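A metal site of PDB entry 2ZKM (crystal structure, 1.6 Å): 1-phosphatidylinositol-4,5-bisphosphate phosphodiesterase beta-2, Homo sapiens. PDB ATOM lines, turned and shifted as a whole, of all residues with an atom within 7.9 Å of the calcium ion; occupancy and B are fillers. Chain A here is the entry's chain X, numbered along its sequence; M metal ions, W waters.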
ATOM      1  N   HIS A 327      26.294  -6.739 -14.750  1.00  0.00           N
ATOM      2  CA  HIS A 327      25.444  -7.758 -15.366  1.00  0.00           C
ATOM      3  C   HIS A 327      24.560  -7.202 -16.491  1.00  0.00           C
ATOM      4  O   HIS A 327      24.022  -6.110 -16.335  1.00  0.00           O
ATOM      5  CB  HIS A 327      24.525  -8.372 -14.314  1.00  0.00           C
ATOM      6  CG  HIS A 327      23.513  -9.315 -14.889  1.00  0.00           C
ATOM      7  ND1 HIS A 327      22.157  -9.052 -14.885  1.00  0.00           N
ATOM      8  CD2 HIS A 327      23.663 -10.505 -15.499  1.00  0.00           C
ATOM      9  CE1 HIS A 327      21.517 -10.051 -15.464  1.00  0.00           C
ATOM     10  NE2 HIS A 327      22.406 -10.946 -15.847  1.00  0.00           N
ATOM     11  N   ASN A 328      24.390  -7.980 -17.582  1.00  0.00           N
ATOM     12  CA  ASN A 328      23.529  -7.632 -18.757  1.00  0.00           C
ATOM     13  C   ASN A 328      23.620  -6.138 -19.059  1.00  0.00           C
ATOM     14  O   ASN A 328      22.640  -5.403 -19.017  1.00  0.00           O
ATOM     15  CB  ASN A 328      22.067  -8.059 -18.557  1.00  0.00           C
ATOM     16  CG  ASN A 328      21.801  -9.500 -18.998  1.00  0.00           C
ATOM     17  OD1 ASN A 328      22.671 -10.179 -19.529  1.00  0.00           O
ATOM     18  ND2 ASN A 328      20.565  -9.960 -18.771  1.00  0.00           N
ATOM     19  N   THR A 329      24.847  -5.734 -19.357  1.00  0.00           N
ATOM     20  CA  THR A 329      25.249  -4.331 -19.315  1.00  0.00           C
ATOM     21  C   THR A 329      24.426  -3.456 -20.248  1.00  0.00           C
ATOM     22  O   THR A 329      24.120  -2.304 -19.934  1.00  0.00           O
ATOM     23  CB  THR A 329      26.744  -4.215 -19.641  1.00  0.00           C
ATOM     24  OG1 THR A 329      27.481  -5.100 -18.786  1.00  0.00           O
ATOM     25  CG2 THR A 329      27.239  -2.792 -19.448  1.00  0.00           C
ATOM     26  N   TYR A 330      24.067  -4.024 -21.399  1.00  0.00           N
ATOM     27  CA  TYR A 330      23.334  -3.329 -22.454  1.00  0.00           C
ATOM     28  C   TYR A 330      21.943  -2.841 -22.041  1.00  0.00           C
ATOM     29  O   TYR A 330      21.357  -2.003 -22.742  1.00  0.00           O
ATOM     30  CB  TYR A 330      23.246  -4.257 -23.678  1.00  0.00           C
ATOM     31  CG  TYR A 330      22.596  -5.598 -23.356  1.00  0.00           C
ATOM     32  CD1 TYR A 330      23.347  -6.672 -22.896  1.00  0.00           C
ATOM     33  CD2 TYR A 330      21.221  -5.770 -23.504  1.00  0.00           C
ATOM     34  CE1 TYR A 330      22.752  -7.896 -22.585  1.00  0.00           C
ATOM     35  CE2 TYR A 330      20.615  -6.970 -23.211  1.00  0.00           C
ATOM     36  CZ  TYR A 330      21.376  -8.034 -22.749  1.00  0.00           C
ATOM     37  OH  TYR A 330      20.738  -9.215 -22.451  1.00  0.00           O
ATOM     38  N   LEU A 331      21.398  -3.356 -20.941  1.00  0.00           N
ATOM     39  CA  LEU A 331      20.046  -2.988 -20.513  1.00  0.00           C
ATOM     40  C   LEU A 331      20.014  -1.719 -19.675  1.00  0.00           C
ATOM     41  O   LEU A 331      20.812  -1.563 -18.747  1.00  0.00           O
ATOM     42  CB  LEU A 331      19.376  -4.133 -19.760  1.00  0.00           C
ATOM     43  CG  LEU A 331      19.063  -5.399 -20.552  1.00  0.00           C
ATOM     44  CD1 LEU A 331      18.523  -6.491 -19.647  1.00  0.00           C
ATOM     45  CD2 LEU A 331      18.071  -5.105 -21.673  1.00  0.00           C
ATOM     46  N   GLN A 335      14.572  -6.304 -17.149  1.00  0.00           N
ATOM     47  CA  GLN A 335      15.152  -7.462 -17.844  1.00  0.00           C
ATOM     48  C   GLN A 335      14.267  -7.990 -18.964  1.00  0.00           C
ATOM     49  O   GLN A 335      14.768  -8.588 -19.911  1.00  0.00           O
ATOM     50  CB  GLN A 335      15.457  -8.594 -16.861  1.00  0.00           C
ATOM     51  CG  GLN A 335      16.461  -8.240 -15.779  1.00  0.00           C
ATOM     52  CD  GLN A 335      17.866  -8.046 -16.318  1.00  0.00           C
ATOM     53  OE1 GLN A 335      18.440  -8.959 -16.932  1.00  0.00           O
ATOM     54  NE2 GLN A 335      18.425  -6.865 -16.101  1.00  0.00           N
ATOM     55  N   GLU A 357      29.007  -7.288 -19.852  1.00  0.00           N
ATOM     56  CA  GLU A 357      28.381  -8.436 -20.492  1.00  0.00           C
ATOM     57  C   GLU A 357      27.747  -8.071 -21.837  1.00  0.00           C
ATOM     58  O   GLU A 357      27.078  -7.038 -21.953  1.00  0.00           O
ATOM     59  CB  GLU A 357      27.340  -9.047 -19.562  1.00  0.00           C
ATOM     60  CG  GLU A 357      26.681 -10.304 -20.096  1.00  0.00           C
ATOM     61  CD  GLU A 357      25.916 -11.045 -19.036  1.00  0.00           C
ATOM     62  OE1 GLU A 357      25.843 -10.563 -17.876  1.00  0.00           O
ATOM     63  OE2 GLU A 357      25.381 -12.130 -19.345  1.00  0.00           O
ATOM     64  N   LEU A 358      27.973  -8.921 -22.829  1.00  0.00           N
ATOM     65  CA  LEU A 358      27.362  -8.779 -24.157  1.00  0.00           C
ATOM     66  C   LEU A 358      26.613 -10.075 -24.468  1.00  0.00           C
ATOM     67  O   LEU A 358      27.244 -11.125 -24.574  1.00  0.00           O
ATOM     68  CB  LEU A 358      28.441  -8.548 -25.234  1.00  0.00           C
ATOM     69  CG  LEU A 358      29.338  -7.296 -25.211  1.00  0.00           C
ATOM     70  CD1 LEU A 358      30.375  -7.356 -24.095  1.00  0.00           C
ATOM     71  CD2 LEU A 358      30.022  -7.107 -26.559  1.00  0.00           C
ATOM     72  N   ASP A 359      25.289  -9.993 -24.597  1.00  0.00           N
ATOM     73  CA  ASP A 359      24.480 -11.145 -24.995  1.00  0.00           C
ATOM     74  C   ASP A 359      24.290 -11.060 -26.504  1.00  0.00           C
ATOM     75  O   ASP A 359      23.574 -10.174 -26.981  1.00  0.00           O
ATOM     76  CB  ASP A 359      23.097 -11.141 -24.326  1.00  0.00           C
ATOM     77  CG  ASP A 359      23.137 -11.472 -22.844  1.00  0.00           C
ATOM     78  OD1 ASP A 359      24.234 -11.675 -22.272  1.00  0.00           O
ATOM     79  OD2 ASP A 359      22.053 -11.542 -22.240  1.00  0.00           O
ATOM     80  N   CYS A 360      24.933 -11.956 -27.233  1.00  0.00           N
ATOM     81  CA  CYS A 360      25.005 -11.843 -28.697  1.00  0.00           C
ATOM     82  C   CYS A 360      24.060 -12.812 -29.403  1.00  0.00           C
ATOM     83  O   CYS A 360      24.040 -14.018 -29.105  1.00  0.00           O
ATOM     84  CB  CYS A 360      26.451 -12.076 -29.162  1.00  0.00           C
ATOM     85  SG  CYS A 360      27.676 -11.109 -28.253  1.00  0.00           S
ATOM     86  N   TRP A 361      23.276 -12.281 -30.339  1.00  0.00           N
ATOM     87  CA  TRP A 361      22.296 -13.069 -31.088  1.00  0.00           C
ATOM     88  C   TRP A 361      22.437 -12.802 -32.573  1.00  0.00           C
ATOM     89  O   TRP A 361      22.959 -11.755 -32.981  1.00  0.00           O
ATOM     90  CB  TRP A 361      20.872 -12.739 -30.620  1.00  0.00           C
ATOM     91  CG  TRP A 361      20.640 -13.041 -29.177  1.00  0.00           C
ATOM     92  CD1 TRP A 361      20.972 -12.253 -28.109  1.00  0.00           C
ATOM     93  CD2 TRP A 361      20.030 -14.228 -28.634  1.00  0.00           C
ATOM     94  NE1 TRP A 361      20.603 -12.873 -26.933  1.00  0.00           N
ATOM     95  CE2 TRP A 361      20.033 -14.085 -27.227  1.00  0.00           C
ATOM     96  CE3 TRP A 361      19.492 -15.389 -29.189  1.00  0.00           C
ATOM     97  CZ2 TRP A 361      19.522 -15.066 -26.375  1.00  0.00           C
ATOM     98  CZ3 TRP A 361      18.983 -16.360 -28.346  1.00  0.00           C
ATOM     99  CH2 TRP A 361      18.998 -16.196 -26.948  1.00  0.00           C
ATOM    100  N   THR A 373      20.922  -8.216 -27.323  1.00  0.00           N
ATOM    101  CA  THR A 373      19.613  -8.067 -26.694  1.00  0.00           C
ATOM    102  C   THR A 373      19.446  -9.174 -25.666  1.00  0.00           C
ATOM    103  O   THR A 373      20.241 -10.114 -25.626  1.00  0.00           O
ATOM    104  CB  THR A 373      18.448  -8.110 -27.726  1.00  0.00           C
ATOM    105  OG1 THR A 373      17.226  -7.696 -27.112  1.00  0.00           O
ATOM    106  CG2 THR A 373      18.269  -9.514 -28.319  1.00  0.00           C
ATOM    107  N   HIS A 374      18.408  -9.067 -24.836  1.00  0.00           N
ATOM    108  CA  HIS A 374      18.042 -10.155 -23.937  1.00  0.00           C
ATOM    109  C   HIS A 374      17.084 -11.074 -24.685  1.00  0.00           C
ATOM    110  O   HIS A 374      15.921 -10.727 -24.931  1.00  0.00           O
ATOM    111  CB  HIS A 374      17.439  -9.611 -22.640  1.00  0.00           C
ATOM    112  CG  HIS A 374      17.397 -10.608 -21.524  1.00  0.00           C
ATOM    113  ND1 HIS A 374      16.799 -10.345 -20.317  1.00  0.00           N
ATOM    114  CD2 HIS A 374      17.881 -11.874 -21.439  1.00  0.00           C
ATOM    115  CE1 HIS A 374      16.907 -11.397 -19.533  1.00  0.00           C
ATOM    116  NE2 HIS A 374      17.560 -12.338 -20.183  1.00  0.00           N
ATOM    117  N   GLY A 375      17.593 -12.238 -25.068  1.00  0.00           N
ATOM    118  CA  GLY A 375      16.813 -13.186 -25.877  1.00  0.00           C
ATOM    119  C   GLY A 375      15.526 -13.627 -25.215  1.00  0.00           C
ATOM    120  O   GLY A 375      15.468 -13.782 -23.990  1.00  0.00           O
ATOM    121  N   SER A 406      32.426 -10.308 -21.013  1.00  0.00           N
ATOM    122  CA  SER A 406      31.716 -11.573 -20.881  1.00  0.00           C
ATOM    123  C   SER A 406      30.714 -11.739 -22.022  1.00  0.00           C
ATOM    124  O   SER A 406      29.636 -11.142 -22.009  1.00  0.00           O
ATOM    125  CB  SER A 406      31.010 -11.636 -19.518  1.00  0.00           C
ATOM    126  OG  SER A 406      30.342 -12.884 -19.370  1.00  0.00           O
ATOM    127  N   PHE A 407      31.080 -12.546 -23.007  1.00  0.00           N
ATOM    128  CA  PHE A 407      30.199 -12.860 -24.128  1.00  0.00           C
ATOM    129  C   PHE A 407      29.260 -13.984 -23.722  1.00  0.00           C
ATOM    130  O   PHE A 407      29.713 -15.034 -23.248  1.00  0.00           O
ATOM    131  CB  PHE A 407      30.992 -13.312 -25.366  1.00  0.00           C
ATOM    132  CG  PHE A 407      31.629 -12.206 -26.157  1.00  0.00           C
ATOM    133  CD1 PHE A 407      32.335 -11.180 -25.538  1.00  0.00           C
ATOM    134  CD2 PHE A 407      31.582 -12.224 -27.542  1.00  0.00           C
ATOM    135  CE1 PHE A 407      32.940 -10.163 -26.283  1.00  0.00           C
ATOM    136  CE2 PHE A 407      32.189 -11.227 -28.297  1.00  0.00           C
ATOM    137  CZ  PHE A 407      32.868 -10.195 -27.676  1.00  0.00           C
ATOM    138  N   GLU A 408      27.959 -13.762 -23.874  1.00  0.00           N
ATOM    139  CA  GLU A 408      26.990 -14.841 -23.789  1.00  0.00           C
ATOM    140  C   GLU A 408      26.527 -15.055 -25.217  1.00  0.00           C
ATOM    141  O   GLU A 408      25.733 -14.280 -25.753  1.00  0.00           O
ATOM    142  CB  GLU A 408      25.823 -14.450 -22.879  1.00  0.00           C
ATOM    143  CG  GLU A 408      24.916 -15.609 -22.546  1.00  0.00           C
ATOM    144  CD  GLU A 408      23.595 -15.139 -21.984  1.00  0.00           C
ATOM    145  OE1 GLU A 408      23.583 -14.568 -20.864  1.00  0.00           O
ATOM    146  OE2 GLU A 408      22.575 -15.343 -22.661  1.00  0.00           O
ATOM    147  N   ASN A 409      27.064 -16.099 -25.841  1.00  0.00           N
ATOM    148  CA  ASN A 409      26.994 -16.239 -27.287  1.00  0.00           C
ATOM    149  C   ASN A 409      25.896 -17.168 -27.770  1.00  0.00           C
ATOM    150  O   ASN A 409      25.845 -18.339 -27.400  1.00  0.00           O
ATOM    151  CB  ASN A 409      28.343 -16.685 -27.850  1.00  0.00           C
ATOM    152  CG  ASN A 409      28.353 -16.740 -29.367  1.00  0.00           C
ATOM    153  OD1 ASN A 409      27.695 -15.940 -30.028  1.00  0.00           O
ATOM    154  ND2 ASN A 409      29.114 -17.674 -29.928  1.00  0.00           N
ATOM    155  N   HIS A 410      25.020 -16.620 -28.601  1.00  0.00           N
ATOM    156  CA  HIS A 410      23.920 -17.366 -29.193  1.00  0.00           C
ATOM    157  C   HIS A 410      23.971 -17.303 -30.703  1.00  0.00           C
ATOM    158  O   HIS A 410      23.021 -17.679 -31.394  1.00  0.00           O
ATOM    159  CB  HIS A 410      22.593 -16.809 -28.695  1.00  0.00           C
ATOM    160  CG  HIS A 410      22.480 -16.819 -27.203  1.00  0.00           C
ATOM    161  ND1 HIS A 410      22.013 -17.916 -26.517  1.00  0.00           N
ATOM    162  CD2 HIS A 410      22.798 -15.892 -26.270  1.00  0.00           C
ATOM    163  CE1 HIS A 410      22.031 -17.647 -25.214  1.00  0.00           C
ATOM    164  NE2 HIS A 410      22.507 -16.438 -25.043  1.00  0.00           N
ATOM    165  N   GLU A 529      19.217 -19.507 -14.373  1.00  0.00           N
ATOM    166  CA  GLU A 529      20.319 -19.093 -15.252  1.00  0.00           C
ATOM    167  C   GLU A 529      19.883 -18.263 -16.464  1.00  0.00           C
ATOM    168  O   GLU A 529      20.693 -17.568 -17.067  1.00  0.00           O
ATOM    169  CB  GLU A 529      21.158 -20.294 -15.687  1.00  0.00           C
ATOM    170  CG  GLU A 529      20.479 -21.226 -16.700  1.00  0.00           C
ATOM    171  CD  GLU A 529      19.667 -22.358 -16.072  1.00  0.00           C
ATOM    172  OE1 GLU A 529      19.141 -22.207 -14.949  1.00  0.00           O
ATOM    173  OE2 GLU A 529      19.555 -23.410 -16.727  1.00  0.00           O
ATOM    174  N   GLY A 530      18.598 -18.341 -16.816  1.00  0.00           N
ATOM    175  CA  GLY A 530      18.090 -17.620 -17.980  1.00  0.00           C
ATOM    176  C   GLY A 530      18.788 -18.033 -19.256  1.00  0.00           C
ATOM    177  O   GLY A 530      19.164 -19.204 -19.421  1.00  0.00           O
ATOM    178  N   THR A 531      19.007 -17.080 -20.158  1.00  0.00           N
ATOM    179  CA  THR A 531      19.566 -17.391 -21.476  1.00  0.00           C
ATOM    180  C   THR A 531      21.004 -17.893 -21.408  1.00  0.00           C
ATOM    181  O   THR A 531      21.497 -18.458 -22.383  1.00  0.00           O
ATOM    182  CB  THR A 531      19.430 -16.220 -22.470  1.00  0.00           C
ATOM    183  OG1 THR A 531      20.061 -15.057 -21.927  1.00  0.00           O
ATOM    184  CG2 THR A 531      17.977 -15.925 -22.759  1.00  0.00           C
ATOM    185  N   ALA A 532      21.670 -17.704 -20.270  1.00  0.00           N
ATOM    186  CA  ALA A 532      23.007 -18.266 -20.066  1.00  0.00           C
ATOM    187  C   ALA A 532      23.023 -19.802 -20.152  1.00  0.00           C
ATOM    188  O   ALA A 532      24.074 -20.406 -20.344  1.00  0.00           O
ATOM    189  CB  ALA A 532      23.581 -17.791 -18.736  1.00  0.00           C
ATOM    190  N   ARG A 598      32.585 -15.817 -11.446  1.00  0.00           N
ATOM    191  CA  ARG A 598      31.683 -14.711 -11.744  1.00  0.00           C
ATOM    192  C   ARG A 598      30.294 -15.078 -11.260  1.00  0.00           C
ATOM    193  O   ARG A 598      29.820 -16.193 -11.517  1.00  0.00           O
ATOM    194  CB  ARG A 598      31.651 -14.403 -13.248  1.00  0.00           C
ATOM    195  CG  ARG A 598      30.734 -13.246 -13.630  1.00  0.00           C
ATOM    196  CD  ARG A 598      30.898 -12.845 -15.105  1.00  0.00           C
ATOM    197  NE  ARG A 598      30.011 -11.725 -15.448  1.00  0.00           N
ATOM    198  CZ  ARG A 598      28.762 -11.851 -15.876  1.00  0.00           C
ATOM    199  NH1 ARG A 598      28.223 -13.048 -16.056  1.00  0.00           N
ATOM    200  NH2 ARG A 598      28.052 -10.765 -16.151  1.00  0.00           N
ATOM    201  N   TYR A 600      26.150 -13.847 -10.999  1.00  0.00           N
ATOM    202  CA  TYR A 600      25.167 -12.977 -11.654  1.00  0.00           C
ATOM    203  C   TYR A 600      23.751 -13.222 -11.109  1.00  0.00           C
ATOM    204  O   TYR A 600      23.489 -14.283 -10.536  1.00  0.00           O
ATOM    205  CB  TYR A 600      25.241 -13.100 -13.181  1.00  0.00           C
ATOM    206  CG  TYR A 600      24.898 -14.464 -13.740  1.00  0.00           C
ATOM    207  CD1 TYR A 600      25.865 -15.475 -13.818  1.00  0.00           C
ATOM    208  CD2 TYR A 600      23.618 -14.746 -14.225  1.00  0.00           C
ATOM    209  CE1 TYR A 600      25.559 -16.716 -14.334  1.00  0.00           C
ATOM    210  CE2 TYR A 600      23.296 -15.990 -14.747  1.00  0.00           C
ATOM    211  CZ  TYR A 600      24.271 -16.975 -14.796  1.00  0.00           C
ATOM    212  OH  TYR A 600      23.985 -18.225 -15.308  1.00  0.00           O
HETATM  213 CA    CA M   1      23.161 -12.384 -20.134  1.00  0.00          CA
HETATM  214  O   HOH W   1      22.671 -12.969 -17.792  1.00  0.00           O
HETATM  215  O   HOH W   2      20.737 -13.053 -19.823  1.00  0.00           O
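The side-chain amide nitrogen (ND2) of Asn 328 is in hydrogen-bond range of the side-chain amide oxygen (OE1) of Gln 335.
The side-chain carboxylate of Glu 408 is in hydrogen-bond range of the side-chain hydroxyl of Thr 531 (2.6 Å).
The backbone NH (N) of Ala 532 is in hydrogen-bond range of the side-chain carboxylate (OE2) of Glu 408 (3.5 Å).
The backbone NH (N) of Glu 408 sits at hydrogen-bond distance from the backbone carbonyl oxygen (O) of Leu 358 (2.8 Å).
The side-chain carboxylate (OE2) of Glu 408 lies within hydrogen-bond range of a ring nitrogen (NE2) of His 410, 2.6 Å away.
The backbone NH of Glu 357 is in hydrogen-bond range of the side-chain hydroxyl of Thr 329 (2.9 Å).
OD2 of Asp 359 lies close to OH of Tyr 330 (2.7 Å).
The backbone carbonyl oxygen of Asp 359 is in hydrogen-bond range of the backbone NH of Thr 373.
Of the 25 residues printed, 4 come within 4 Å of the calcium ion.
Along chain A the residues within 4 Å of the calcium ion span positions 328 to 408.
The nearest printed residue that does not touch the calcium ion is Thr 531 (4.5 Å).
The calcium ion is bound by the side-chain amide oxygen (OD1) of Asn 328 (2.3 Å), the side-chain carboxylate (OE1) of Glu 408 (2.3 Å), the side-chain carboxylate (OE2) of Glu 357 (2.4 Å), water W1 (2.5 Å), the side-chain carboxylate (OD1) of Asp 359 (2.5 Å), the side-chain carboxylate (OD2) of Asp 359 (2.5 Å) and water W2 (2.5 Å).
The calcium ion has seven donor atoms within binding distance.
Water W2 lies within hydrogen-bond range of the side-chain hydroxyl of Thr 531, the side-chain amide nitrogen of Asn 328 and a ring nitrogen (NE2) of His 374.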
